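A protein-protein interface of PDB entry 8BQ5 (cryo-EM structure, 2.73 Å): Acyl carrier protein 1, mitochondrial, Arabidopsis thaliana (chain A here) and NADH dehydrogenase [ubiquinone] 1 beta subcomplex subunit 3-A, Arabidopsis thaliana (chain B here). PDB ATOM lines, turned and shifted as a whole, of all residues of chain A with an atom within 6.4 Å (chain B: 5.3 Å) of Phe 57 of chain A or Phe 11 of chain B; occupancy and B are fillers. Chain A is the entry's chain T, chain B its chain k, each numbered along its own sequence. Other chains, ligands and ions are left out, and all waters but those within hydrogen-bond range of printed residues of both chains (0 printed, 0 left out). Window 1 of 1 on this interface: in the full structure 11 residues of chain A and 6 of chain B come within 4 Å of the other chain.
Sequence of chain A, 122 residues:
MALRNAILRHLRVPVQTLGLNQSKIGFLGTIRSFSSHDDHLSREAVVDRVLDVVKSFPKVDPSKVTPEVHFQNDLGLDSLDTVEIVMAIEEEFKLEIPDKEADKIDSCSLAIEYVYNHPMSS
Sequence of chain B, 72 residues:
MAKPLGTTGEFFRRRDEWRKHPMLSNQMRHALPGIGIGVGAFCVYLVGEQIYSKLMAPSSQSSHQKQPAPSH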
ATOM      1  N   ASP A  52     -11.431  -6.869 -17.891  1.00  0.00           N
ATOM      2  CA  ASP A  52     -10.068  -6.863 -17.296  1.00  0.00           C
ATOM      3  C   ASP A  52      -9.938  -7.986 -16.258  1.00  0.00           C
ATOM      4  O   ASP A  52      -8.891  -8.634 -16.247  1.00  0.00           O
ATOM      5  CB  ASP A  52      -9.707  -5.487 -16.726  1.00  0.00           C
ATOM      6  CG  ASP A  52      -9.772  -4.367 -17.749  1.00  0.00           C
ATOM      7  OD1 ASP A  52      -9.927  -4.672 -18.949  1.00  0.00           O
ATOM      8  OD2 ASP A  52      -9.672  -3.196 -17.337  1.00  0.00           O
ATOM      9  N   VAL A  53     -10.973  -8.214 -15.445  1.00  0.00           N
ATOM     10  CA  VAL A  53     -10.946  -9.290 -14.408  1.00  0.00           C
ATOM     11  C   VAL A  53     -10.767 -10.647 -15.095  1.00  0.00           C
ATOM     12  O   VAL A  53     -10.008 -11.480 -14.566  1.00  0.00           O
ATOM     13  CB  VAL A  53     -12.223  -9.273 -13.547  1.00  0.00           C
ATOM     14  CG1 VAL A  53     -12.221 -10.374 -12.500  1.00  0.00           C
ATOM     15  CG2 VAL A  53     -12.481  -7.921 -12.906  1.00  0.00           C
ATOM     16  N   VAL A  54     -11.467 -10.865 -16.209  1.00  0.00           N
ATOM     17  CA  VAL A  54     -11.341 -12.124 -16.938  1.00  0.00           C
ATOM     18  C   VAL A  54     -10.018 -12.174 -17.692  1.00  0.00           C
ATOM     19  O   VAL A  54      -9.480 -13.255 -17.963  1.00  0.00           O
ATOM     20  CB  VAL A  54     -12.549 -12.320 -17.873  1.00  0.00           C
ATOM     21  CG1 VAL A  54     -12.553 -13.722 -18.455  1.00  0.00           C
ATOM     22  CG2 VAL A  54     -13.842 -12.061 -17.118  1.00  0.00           C
ATOM     23  N   LYS A  55      -9.475 -11.007 -18.048  1.00  0.00           N
ATOM     24  CA  LYS A  55      -8.146 -10.955 -18.649  1.00  0.00           C
ATOM     25  C   LYS A  55      -7.072 -11.433 -17.685  1.00  0.00           C
ATOM     26  O   LYS A  55      -6.157 -12.164 -18.083  1.00  0.00           O
ATOM     27  CB  LYS A  55      -7.828  -9.530 -19.099  1.00  0.00           C
ATOM     28  CG  LYS A  55      -7.913  -9.290 -20.592  1.00  0.00           C
ATOM     29  CD  LYS A  55      -7.731  -7.811 -20.889  1.00  0.00           C
ATOM     30  CE  LYS A  55      -8.289  -7.437 -22.249  1.00  0.00           C
ATOM     31  NZ  LYS A  55      -7.224  -7.373 -23.284  1.00  0.00           N
ATOM     32  N   SER A  56      -7.170 -11.043 -16.413  1.00  0.00           N
ATOM     33  CA  SER A  56      -6.086 -11.218 -15.455  1.00  0.00           C
ATOM     34  C   SER A  56      -5.907 -12.657 -14.994  1.00  0.00           C
ATOM     35  O   SER A  56      -5.175 -12.888 -14.026  1.00  0.00           O
ATOM     36  CB  SER A  56      -6.322 -10.329 -14.232  1.00  0.00           C
ATOM     37  OG  SER A  56      -6.264  -8.958 -14.581  1.00  0.00           O
ATOM     38  N   PHE A  57      -6.547 -13.620 -15.639  1.00  0.00           N
ATOM     39  CA  PHE A  57      -6.424 -14.999 -15.191  1.00  0.00           C
ATOM     40  C   PHE A  57      -5.260 -15.681 -15.903  1.00  0.00           C
ATOM     41  O   PHE A  57      -5.134 -15.560 -17.128  1.00  0.00           O
ATOM     42  CB  PHE A  57      -7.721 -15.766 -15.426  1.00  0.00           C
ATOM     43  CG  PHE A  57      -7.791 -17.054 -14.663  1.00  0.00           C
ATOM     44  CD1 PHE A  57      -8.199 -18.218 -15.267  1.00  0.00           C
ATOM     45  CD2 PHE A  57      -7.437 -17.096 -13.329  1.00  0.00           C
ATOM     46  CE1 PHE A  57      -8.247 -19.394 -14.550  1.00  0.00           C
ATOM     47  CE2 PHE A  57      -7.462 -18.276 -12.623  1.00  0.00           C
ATOM     48  CZ  PHE A  57      -7.880 -19.425 -13.235  1.00  0.00           C
ATOM     49  N   PRO A  58      -4.386 -16.387 -15.174  1.00  0.00           N
ATOM     50  CA  PRO A  58      -3.218 -17.011 -15.818  1.00  0.00           C
ATOM     51  C   PRO A  58      -3.545 -17.894 -17.008  1.00  0.00           C
ATOM     52  O   PRO A  58      -2.915 -17.748 -18.062  1.00  0.00           O
ATOM     53  CB  PRO A  58      -2.586 -17.820 -14.675  1.00  0.00           C
ATOM     54  CG  PRO A  58      -3.596 -17.826 -13.557  1.00  0.00           C
ATOM     55  CD  PRO A  58      -4.368 -16.576 -13.716  1.00  0.00           C
ATOM     56  N   LYS A  59      -4.519 -18.798 -16.882  1.00  0.00           N
ATOM     57  CA  LYS A  59      -4.774 -19.747 -17.961  1.00  0.00           C
ATOM     58  C   LYS A  59      -5.484 -19.082 -19.135  1.00  0.00           C
ATOM     59  O   LYS A  59      -5.347 -19.523 -20.282  1.00  0.00           O
ATOM     60  CB  LYS A  59      -5.576 -20.936 -17.436  1.00  0.00           C
ATOM     61  CG  LYS A  59      -4.746 -21.874 -16.566  1.00  0.00           C
ATOM     62  CD  LYS A  59      -5.533 -22.421 -15.389  1.00  0.00           C
ATOM     63  CE  LYS A  59      -6.897 -22.919 -15.814  1.00  0.00           C
ATOM     64  NZ  LYS A  59      -7.322 -24.138 -15.079  1.00  0.00           N
ATOM     65  N   VAL A  60      -6.245 -18.018 -18.873  1.00  0.00           N
ATOM     66  CA  VAL A  60      -6.887 -17.281 -19.955  1.00  0.00           C
ATOM     67  C   VAL A  60      -5.864 -16.389 -20.640  1.00  0.00           C
ATOM     68  O   VAL A  60      -5.173 -15.594 -19.990  1.00  0.00           O
ATOM     69  CB  VAL A  60      -8.067 -16.457 -19.419  1.00  0.00           C
ATOM     70  CG1 VAL A  60      -8.914 -15.929 -20.566  1.00  0.00           C
ATOM     71  CG2 VAL A  60      -8.906 -17.290 -18.483  1.00  0.00           C
ATOM     72  N   ASP A  61      -5.762 -16.518 -21.961  1.00  0.00           N
ATOM     73  CA  ASP A  61      -4.878 -15.669 -22.750  1.00  0.00           C
ATOM     74  C   ASP A  61      -5.593 -14.373 -23.107  1.00  0.00           C
ATOM     75  O   ASP A  61      -6.696 -14.423 -23.670  1.00  0.00           O
ATOM     76  CB  ASP A  61      -4.430 -16.386 -24.011  1.00  0.00           C
ATOM     77  CG  ASP A  61      -3.736 -17.700 -23.714  1.00  0.00           C
ATOM     78  OD1 ASP A  61      -4.041 -18.311 -22.668  1.00  0.00           O
ATOM     79  OD2 ASP A  61      -2.880 -18.117 -24.521  1.00  0.00           O
ATOM     80  N   PRO A  62      -5.013 -13.206 -22.817  1.00  0.00           N
ATOM     81  CA  PRO A  62      -5.750 -11.947 -22.985  1.00  0.00           C
ATOM     82  C   PRO A  62      -5.827 -11.476 -24.428  1.00  0.00           C
ATOM     83  O   PRO A  62      -5.433 -10.346 -24.735  1.00  0.00           O
ATOM     84  CB  PRO A  62      -4.950 -10.953 -22.126  1.00  0.00           C
ATOM     85  CG  PRO A  62      -3.890 -11.776 -21.412  1.00  0.00           C
ATOM     86  CD  PRO A  62      -3.670 -12.976 -22.265  1.00  0.00           C
ATOM     87  N   LEU A  77     -11.446 -23.272 -19.382  1.00  0.00           N
ATOM     88  CA  LEU A  77     -11.165 -23.314 -17.954  1.00  0.00           C
ATOM     89  C   LEU A  77     -12.004 -24.402 -17.300  1.00  0.00           C
ATOM     90  O   LEU A  77     -13.028 -24.830 -17.840  1.00  0.00           O
ATOM     91  CB  LEU A  77     -11.475 -21.979 -17.246  1.00  0.00           C
ATOM     92  CG  LEU A  77     -10.679 -20.697 -17.506  1.00  0.00           C
ATOM     93  CD1 LEU A  77      -9.233 -20.901 -17.198  1.00  0.00           C
ATOM     94  CD2 LEU A  77     -10.839 -20.190 -18.906  1.00  0.00           C
ATOM     95  N   ASP A  81     -12.226 -22.789 -11.759  1.00  0.00           N
ATOM     96  CA  ASP A  81     -11.628 -21.547 -12.236  1.00  0.00           C
ATOM     97  C   ASP A  81     -12.682 -20.458 -12.386  1.00  0.00           C
ATOM     98  O   ASP A  81     -12.418 -19.284 -12.105  1.00  0.00           O
ATOM     99  CB  ASP A  81     -10.912 -21.778 -13.567  1.00  0.00           C
ATOM    100  CG  ASP A  81     -10.116 -23.066 -13.589  1.00  0.00           C
ATOM    101  OD1 ASP A  81      -9.616 -23.482 -12.522  1.00  0.00           O
ATOM    102  OD2 ASP A  81      -9.982 -23.660 -14.677  1.00  0.00           O
ATOM    103  N   THR A  82     -13.882 -20.834 -12.832  1.00  0.00           N
ATOM    104  CA  THR A  82     -14.962 -19.865 -13.004  1.00  0.00           C
ATOM    105  C   THR A  82     -15.352 -19.230 -11.676  1.00  0.00           C
ATOM    106  O   THR A  82     -15.608 -18.021 -11.611  1.00  0.00           O
ATOM    107  CB  THR A  82     -16.171 -20.545 -13.646  1.00  0.00           C
ATOM    108  OG1 THR A  82     -15.767 -21.182 -14.865  1.00  0.00           O
ATOM    109  CG2 THR A  82     -17.267 -19.532 -13.940  1.00  0.00           C
ATOM    110  N   GLU A  84     -13.499 -18.651  -9.083  1.00  0.00           N
ATOM    111  CA  GLU A  84     -12.506 -17.632  -8.764  1.00  0.00           C
ATOM    112  C   GLU A  84     -12.745 -16.365  -9.572  1.00  0.00           C
ATOM    113  O   GLU A  84     -12.584 -15.252  -9.058  1.00  0.00           O
ATOM    114  CB  GLU A  84     -11.102 -18.180  -9.016  1.00  0.00           C
ATOM    115  CG  GLU A  84     -10.704 -19.294  -8.069  1.00  0.00           C
ATOM    116  CD  GLU A  84      -9.887 -20.372  -8.752  1.00  0.00           C
ATOM    117  OE1 GLU A  84      -9.713 -20.292  -9.985  1.00  0.00           O
ATOM    118  OE2 GLU A  84      -9.423 -21.300  -8.059  1.00  0.00           O
ATOM    119  N   ILE A  85     -13.133 -16.514 -10.840  1.00  0.00           N
ATOM    120  CA  ILE A  85     -13.455 -15.352 -11.661  1.00  0.00           C
ATOM    121  C   ILE A  85     -14.644 -14.603 -11.076  1.00  0.00           C
ATOM    122  O   ILE A  85     -14.651 -13.367 -11.022  1.00  0.00           O
ATOM    123  CB  ILE A  85     -13.715 -15.775 -13.118  1.00  0.00           C
ATOM    124  CG1 ILE A  85     -12.531 -16.575 -13.669  1.00  0.00           C
ATOM    125  CG2 ILE A  85     -13.979 -14.559 -13.991  1.00  0.00           C
ATOM    126  CD1 ILE A  85     -11.177 -15.980 -13.351  1.00  0.00           C
ATOM    127  N   VAL A  86     -15.665 -15.335 -10.629  1.00  0.00           N
ATOM    128  CA  VAL A  86     -16.835 -14.694 -10.040  1.00  0.00           C
ATOM    129  C   VAL A  86     -16.450 -13.942  -8.772  1.00  0.00           C
ATOM    130  O   VAL A  86     -16.842 -12.786  -8.581  1.00  0.00           O
ATOM    131  CB  VAL A  86     -17.935 -15.738  -9.773  1.00  0.00           C
ATOM    132  CG1 VAL A  86     -19.076 -15.121  -8.983  1.00  0.00           C
ATOM    133  CG2 VAL A  86     -18.438 -16.320 -11.081  1.00  0.00           C
ATOM    134  N   MET A  87     -15.652 -14.573  -7.904  1.00  0.00           N
ATOM    135  CA  MET A  87     -15.247 -13.933  -6.655  1.00  0.00           C
ATOM    136  C   MET A  87     -14.461 -12.656  -6.915  1.00  0.00           C
ATOM    137  O   MET A  87     -14.638 -11.654  -6.213  1.00  0.00           O
ATOM    138  CB  MET A  87     -14.419 -14.901  -5.811  1.00  0.00           C
ATOM    139  CG  MET A  87     -14.425 -14.580  -4.325  1.00  0.00           C
ATOM    140  SD  MET A  87     -13.649 -15.852  -3.311  1.00  0.00           S
ATOM    141  CE  MET A  87     -12.138 -15.017  -2.839  1.00  0.00           C
ATOM    142  N   ALA A  88     -13.573 -12.676  -7.911  1.00  0.00           N
ATOM    143  CA  ALA A  88     -12.828 -11.471  -8.254  1.00  0.00           C
ATOM    144  C   ALA A  88     -13.737 -10.420  -8.884  1.00  0.00           C
ATOM    145  O   ALA A  88     -13.442  -9.222  -8.824  1.00  0.00           O
ATOM    146  CB  ALA A  88     -11.668 -11.819  -9.183  1.00  0.00           C
ATOM    147  N   ILE A  89     -14.838 -10.851  -9.505  1.00  0.00           N
ATOM    148  CA  ILE A  89     -15.843  -9.896  -9.968  1.00  0.00           C
ATOM    149  C   ILE A  89     -16.576  -9.285  -8.779  1.00  0.00           C
ATOM    150  O   ILE A  89     -16.864  -8.081  -8.760  1.00  0.00           O
ATOM    151  CB  ILE A  89     -16.816 -10.569 -10.956  1.00  0.00           C
ATOM    152  CG1 ILE A  89     -16.137 -10.786 -12.309  1.00  0.00           C
ATOM    153  CG2 ILE A  89     -18.072  -9.734 -11.135  1.00  0.00           C
ATOM    154  CD1 ILE A  89     -16.687 -11.960 -13.084  1.00  0.00           C
ATOM    155  N   GLY B   6       0.453 -20.938  -6.570  1.00  0.00           N
ATOM    156  CA  GLY B   6      -0.587 -21.678  -7.317  1.00  0.00           C
ATOM    157  C   GLY B   6      -1.424 -20.837  -8.274  1.00  0.00           C
ATOM    158  O   GLY B   6      -1.225 -19.610  -8.328  1.00  0.00           O
ATOM    159  N   THR B   7      -2.338 -21.485  -9.011  1.00  0.00           N
ATOM    160  CA  THR B   7      -3.207 -20.768  -9.992  1.00  0.00           C
ATOM    161  C   THR B   7      -4.092 -19.767  -9.251  1.00  0.00           C
ATOM    162  O   THR B   7      -3.900 -18.558  -9.467  1.00  0.00           O
ATOM    163  CB  THR B   7      -4.086 -21.738 -10.798  1.00  0.00           C
ATOM    164  OG1 THR B   7      -3.259 -22.710 -11.437  1.00  0.00           O
ATOM    165  CG2 THR B   7      -4.926 -21.043 -11.844  1.00  0.00           C
ATOM    166  N   THR B   8      -5.030 -20.254  -8.430  1.00  0.00           N
ATOM    167  CA  THR B   8      -5.918 -19.376  -7.622  1.00  0.00           C
ATOM    168  C   THR B   8      -5.090 -18.271  -6.964  1.00  0.00           C
ATOM    169  O   THR B   8      -5.486 -17.089  -7.069  1.00  0.00           O
ATOM    170  CB  THR B   8      -6.565 -20.159  -6.474  1.00  0.00           C
ATOM    171  OG1 THR B   8      -7.018 -21.421  -6.964  1.00  0.00           O
ATOM    172  CG2 THR B   8      -7.708 -19.420  -5.814  1.00  0.00           C
ATOM    173  N   GLY B   9      -3.993 -18.643  -6.300  1.00  0.00           N
ATOM    174  CA  GLY B   9      -3.184 -17.648  -5.571  1.00  0.00           C
ATOM    175  C   GLY B   9      -2.674 -16.537  -6.467  1.00  0.00           C
ATOM    176  O   GLY B   9      -2.951 -15.365  -6.152  1.00  0.00           O
ATOM    177  N   GLU B  10      -1.964 -16.886  -7.544  1.00  0.00           N
ATOM    178  CA  GLU B  10      -1.369 -15.862  -8.452  1.00  0.00           C
ATOM    179  C   GLU B  10      -2.486 -15.056  -9.124  1.00  0.00           C
ATOM    180  O   GLU B  10      -2.276 -13.860  -9.360  1.00  0.00           O
ATOM    181  CB  GLU B  10      -0.449 -16.523  -9.482  1.00  0.00           C
ATOM    182  CG  GLU B  10       0.409 -15.553 -10.281  1.00  0.00           C
ATOM    183  CD  GLU B  10       1.130 -14.457  -9.509  1.00  0.00           C
ATOM    184  OE1 GLU B  10       1.882 -14.786  -8.572  1.00  0.00           O
ATOM    185  OE2 GLU B  10       0.950 -13.276  -9.861  1.00  0.00           O
ATOM    186  N   PHE B  11      -3.627 -15.682  -9.408  1.00  0.00           N
ATOM    187  CA  PHE B  11      -4.768 -14.933  -9.996  1.00  0.00           C
ATOM    188  C   PHE B  11      -5.113 -13.747  -9.101  1.00  0.00           C
ATOM    189  O   PHE B  11      -5.204 -12.620  -9.612  1.00  0.00           O
ATOM    190  CB  PHE B  11      -5.991 -15.832 -10.161  1.00  0.00           C
ATOM    191  CG  PHE B  11      -7.242 -15.089 -10.548  1.00  0.00           C
ATOM    192  CD1 PHE B  11      -7.242 -14.203 -11.614  1.00  0.00           C
ATOM    193  CD2 PHE B  11      -8.417 -15.266  -9.840  1.00  0.00           C
ATOM    194  CE1 PHE B  11      -8.390 -13.517 -11.974  1.00  0.00           C
ATOM    195  CE2 PHE B  11      -9.563 -14.579 -10.199  1.00  0.00           C
ATOM    196  CZ  PHE B  11      -9.547 -13.705 -11.261  1.00  0.00           C
ATOM    197  N   PHE B  12      -5.286 -14.001  -7.804  1.00  0.00           N
ATOM    198  CA  PHE B  12      -5.693 -12.920  -6.867  1.00  0.00           C
ATOM    199  C   PHE B  12      -4.535 -11.941  -6.681  1.00  0.00           C
ATOM    200  O   PHE B  12      -4.815 -10.749  -6.517  1.00  0.00           O
ATOM    201  CB  PHE B  12      -6.227 -13.524  -5.570  1.00  0.00           C
ATOM    202  CG  PHE B  12      -7.620 -14.082  -5.729  1.00  0.00           C
ATOM    203  CD1 PHE B  12      -8.666 -13.265  -6.122  1.00  0.00           C
ATOM    204  CD2 PHE B  12      -7.881 -15.427  -5.522  1.00  0.00           C
ATOM    205  CE1 PHE B  12      -9.946 -13.774  -6.285  1.00  0.00           C
ATOM    206  CE2 PHE B  12      -9.160 -15.936  -5.687  1.00  0.00           C
ATOM    207  CZ  PHE B  12     -10.189 -15.110  -6.071  1.00  0.00           C
ATOM    208  N   ARG B  13      -3.291 -12.416  -6.764  1.00  0.00           N
ATOM    209  CA  ARG B  13      -2.137 -11.486  -6.691  1.00  0.00           C
ATOM    210  C   ARG B  13      -2.214 -10.516  -7.873  1.00  0.00           C
ATOM    211  O   ARG B  13      -1.925  -9.323  -7.667  1.00  0.00           O
ATOM    212  CB  ARG B  13      -0.825 -12.272  -6.650  1.00  0.00           C
ATOM    213  CG  ARG B  13       0.398 -11.375  -6.550  1.00  0.00           C
ATOM    214  CD  ARG B  13       1.694 -12.146  -6.437  1.00  0.00           C
ATOM    215  NE  ARG B  13       2.865 -11.289  -6.318  1.00  0.00           N
ATOM    216  CZ  ARG B  13       4.082 -11.724  -6.018  1.00  0.00           C
ATOM    217  NH1 ARG B  13       4.290 -13.011  -5.799  1.00  0.00           N
ATOM    218  NH2 ARG B  13       5.086 -10.871  -5.933  1.00  0.00           N
ATOM    219  N   ARG B  14      -2.607 -11.005  -9.052  1.00  0.00           N
ATOM    220  CA  ARG B  14      -2.770 -10.128 -10.244  1.00  0.00           C
ATOM    221  C   ARG B  14      -3.912  -9.129 -10.022  1.00  0.00           C
ATOM    222  O   ARG B  14      -3.771  -7.979 -10.480  1.00  0.00           O
ATOM    223  CB  ARG B  14      -2.995 -10.987 -11.492  1.00  0.00           C
ATOM    224  CG  ARG B  14      -1.754 -11.731 -11.959  1.00  0.00           C
ATOM    225  CD  ARG B  14      -2.046 -12.596 -13.169  1.00  0.00           C
ATOM    226  NE  ARG B  14      -1.425 -13.909 -13.090  1.00  0.00           N
ATOM    227  CZ  ARG B  14      -0.632 -14.429 -14.021  1.00  0.00           C
ATOM    228  NH1 ARG B  14      -0.355 -13.747 -15.120  1.00  0.00           N
ATOM    229  NH2 ARG B  14      -0.115 -15.631 -13.851  1.00  0.00           N
ATOM    230  N   ARG B  15      -5.003  -9.550  -9.374  1.00  0.00           N
ATOM    231  CA  ARG B  15      -6.136  -8.667  -9.129  1.00  0.00           C
ATOM    232  C   ARG B  15      -5.807  -7.558  -8.137  1.00  0.00           C
ATOM    233  O   ARG B  15      -6.393  -6.474  -8.225  1.00  0.00           O
ATOM    234  CB  ARG B  15      -7.335  -9.476  -8.633  1.00  0.00           C
ATOM    235  CG  ARG B  15      -7.853 -10.489  -9.641  1.00  0.00           C
ATOM    236  CD  ARG B  15      -8.211  -9.799 -10.943  1.00  0.00           C
ATOM    237  NE  ARG B  15      -8.982  -8.582 -10.720  1.00  0.00           N
ATOM    238  CZ  ARG B  15      -9.141  -7.624 -11.621  1.00  0.00           C
ATOM    239  NH1 ARG B  15      -8.554  -7.685 -12.804  1.00  0.00           N
ATOM    240  NH2 ARG B  15      -9.896  -6.571 -11.323  1.00  0.00           N
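OG of Ser 56 of chain A lies within hydrogen-bond range of O of Asp 52 of chain A, 3.1 Å away. The side-chain amino group (NZ) of Lys 59 of chain A lies within salt-bridge range of the side-chain carboxylate (OD2) of Asp 81 of chain A (2.7 Å).
Among the printed residues, merely in contact across the chains: Ser 56 of chain A with Arg 14 of chain B (3.3 Å), Val 53 of chain A with Arg 15 of chain B (3.3 Å), Glu 84 of chain A with Phe 11 of chain B (3.3 Å), Phe 57 of chain A with Phe 11 of chain B (3.4 Å), Pro 58 of chain A with Arg 14 of chain B (3.4 Å), Ser 56 of chain A with Phe 11 of chain B (3.4 Å), Ile 85 of chain A with Phe 11 of chain B (3.5 Å), Ala 88 of chain A with Phe 11 of chain B (3.5 Å), Asp 52 of chain A with Arg 15 of chain B (3.6 Å), Phe 57 of chain A with Thr 7 of chain B (3.6 Å), Val 53 of chain A with Phe 11 of chain B (3.7 Å), Met 87 of chain A with Phe 12 of chain B (3.8 Å), Glu 84 of chain A with Phe 12 of chain B (3.8 Å), Lys 59 of chain A with Thr 7 of chain B (3.9 Å), Pro 58 of chain A with Thr 7 of chain B (3.9 Å), Ala 88 of chain A with Phe 12 of chain B (3.9 Å) and Pro 58 of chain A with Phe 11 of chain B (3.98 Å).
OE2 of Glu 84 of chain A lies within hydrogen-bond range of OG1 of Thr 8 of chain B. The side-chain hydroxyl (OG) of Ser 56 of chain A lies within hydrogen-bond range of the guanidinium group (NH1) of Arg 15 of chain B (3.2 Å).
Of the printed residues of chain B, Val 53 of chain A touches Phe 11 and Arg 15. Phe 57 of chain A touches two residues of chain B. Of the printed residues of chain B, Ile 85 of chain A touches Phe 11. Of the printed residues of chain B, Ala 88 of chain A touches Phe 11 and Phe 12. Gly 9 of chain B touches none of the printed residues of chain A. Printed residues of chain A within 4 Å of Phe 12 of chain B: Glu 84, Met 87 and Ala 88. Of the printed residues of chain A, Arg 15 of chain B touches Asp 52, Val 53 and Ser 56. The nearest residue of chain B that does not touch Phe 57 of chain A is Arg 14 of chain B (5.1 Å). The nearest residue of chain A that does not touch Phe 11 of chain B is Asp 81 of chain A (5.8 Å).
Hydrophobic or aromatic side chains of chain A within 4 Å of the printed part of chain B: Val 53, Phe 57, Pro 58, Ile 85, Met 87 and Ala 88. Printed residues of chain B that touch a printed residue of chain A: Thr 7, Thr 8, Phe 11, Phe 12, Arg 14 and Arg 15. Hydrophobic or aromatic side chains of chain B within 4 Å of the printed part of chain A: Phe 11 and Phe 12. Along chain B the printed residues that touch a printed residue of chain A span positions 7 to 15. Among the printed residues, no Asp or Glu carboxylate lies within 4 Å of a Lys or Arg side-chain nitrogen of the other chain.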
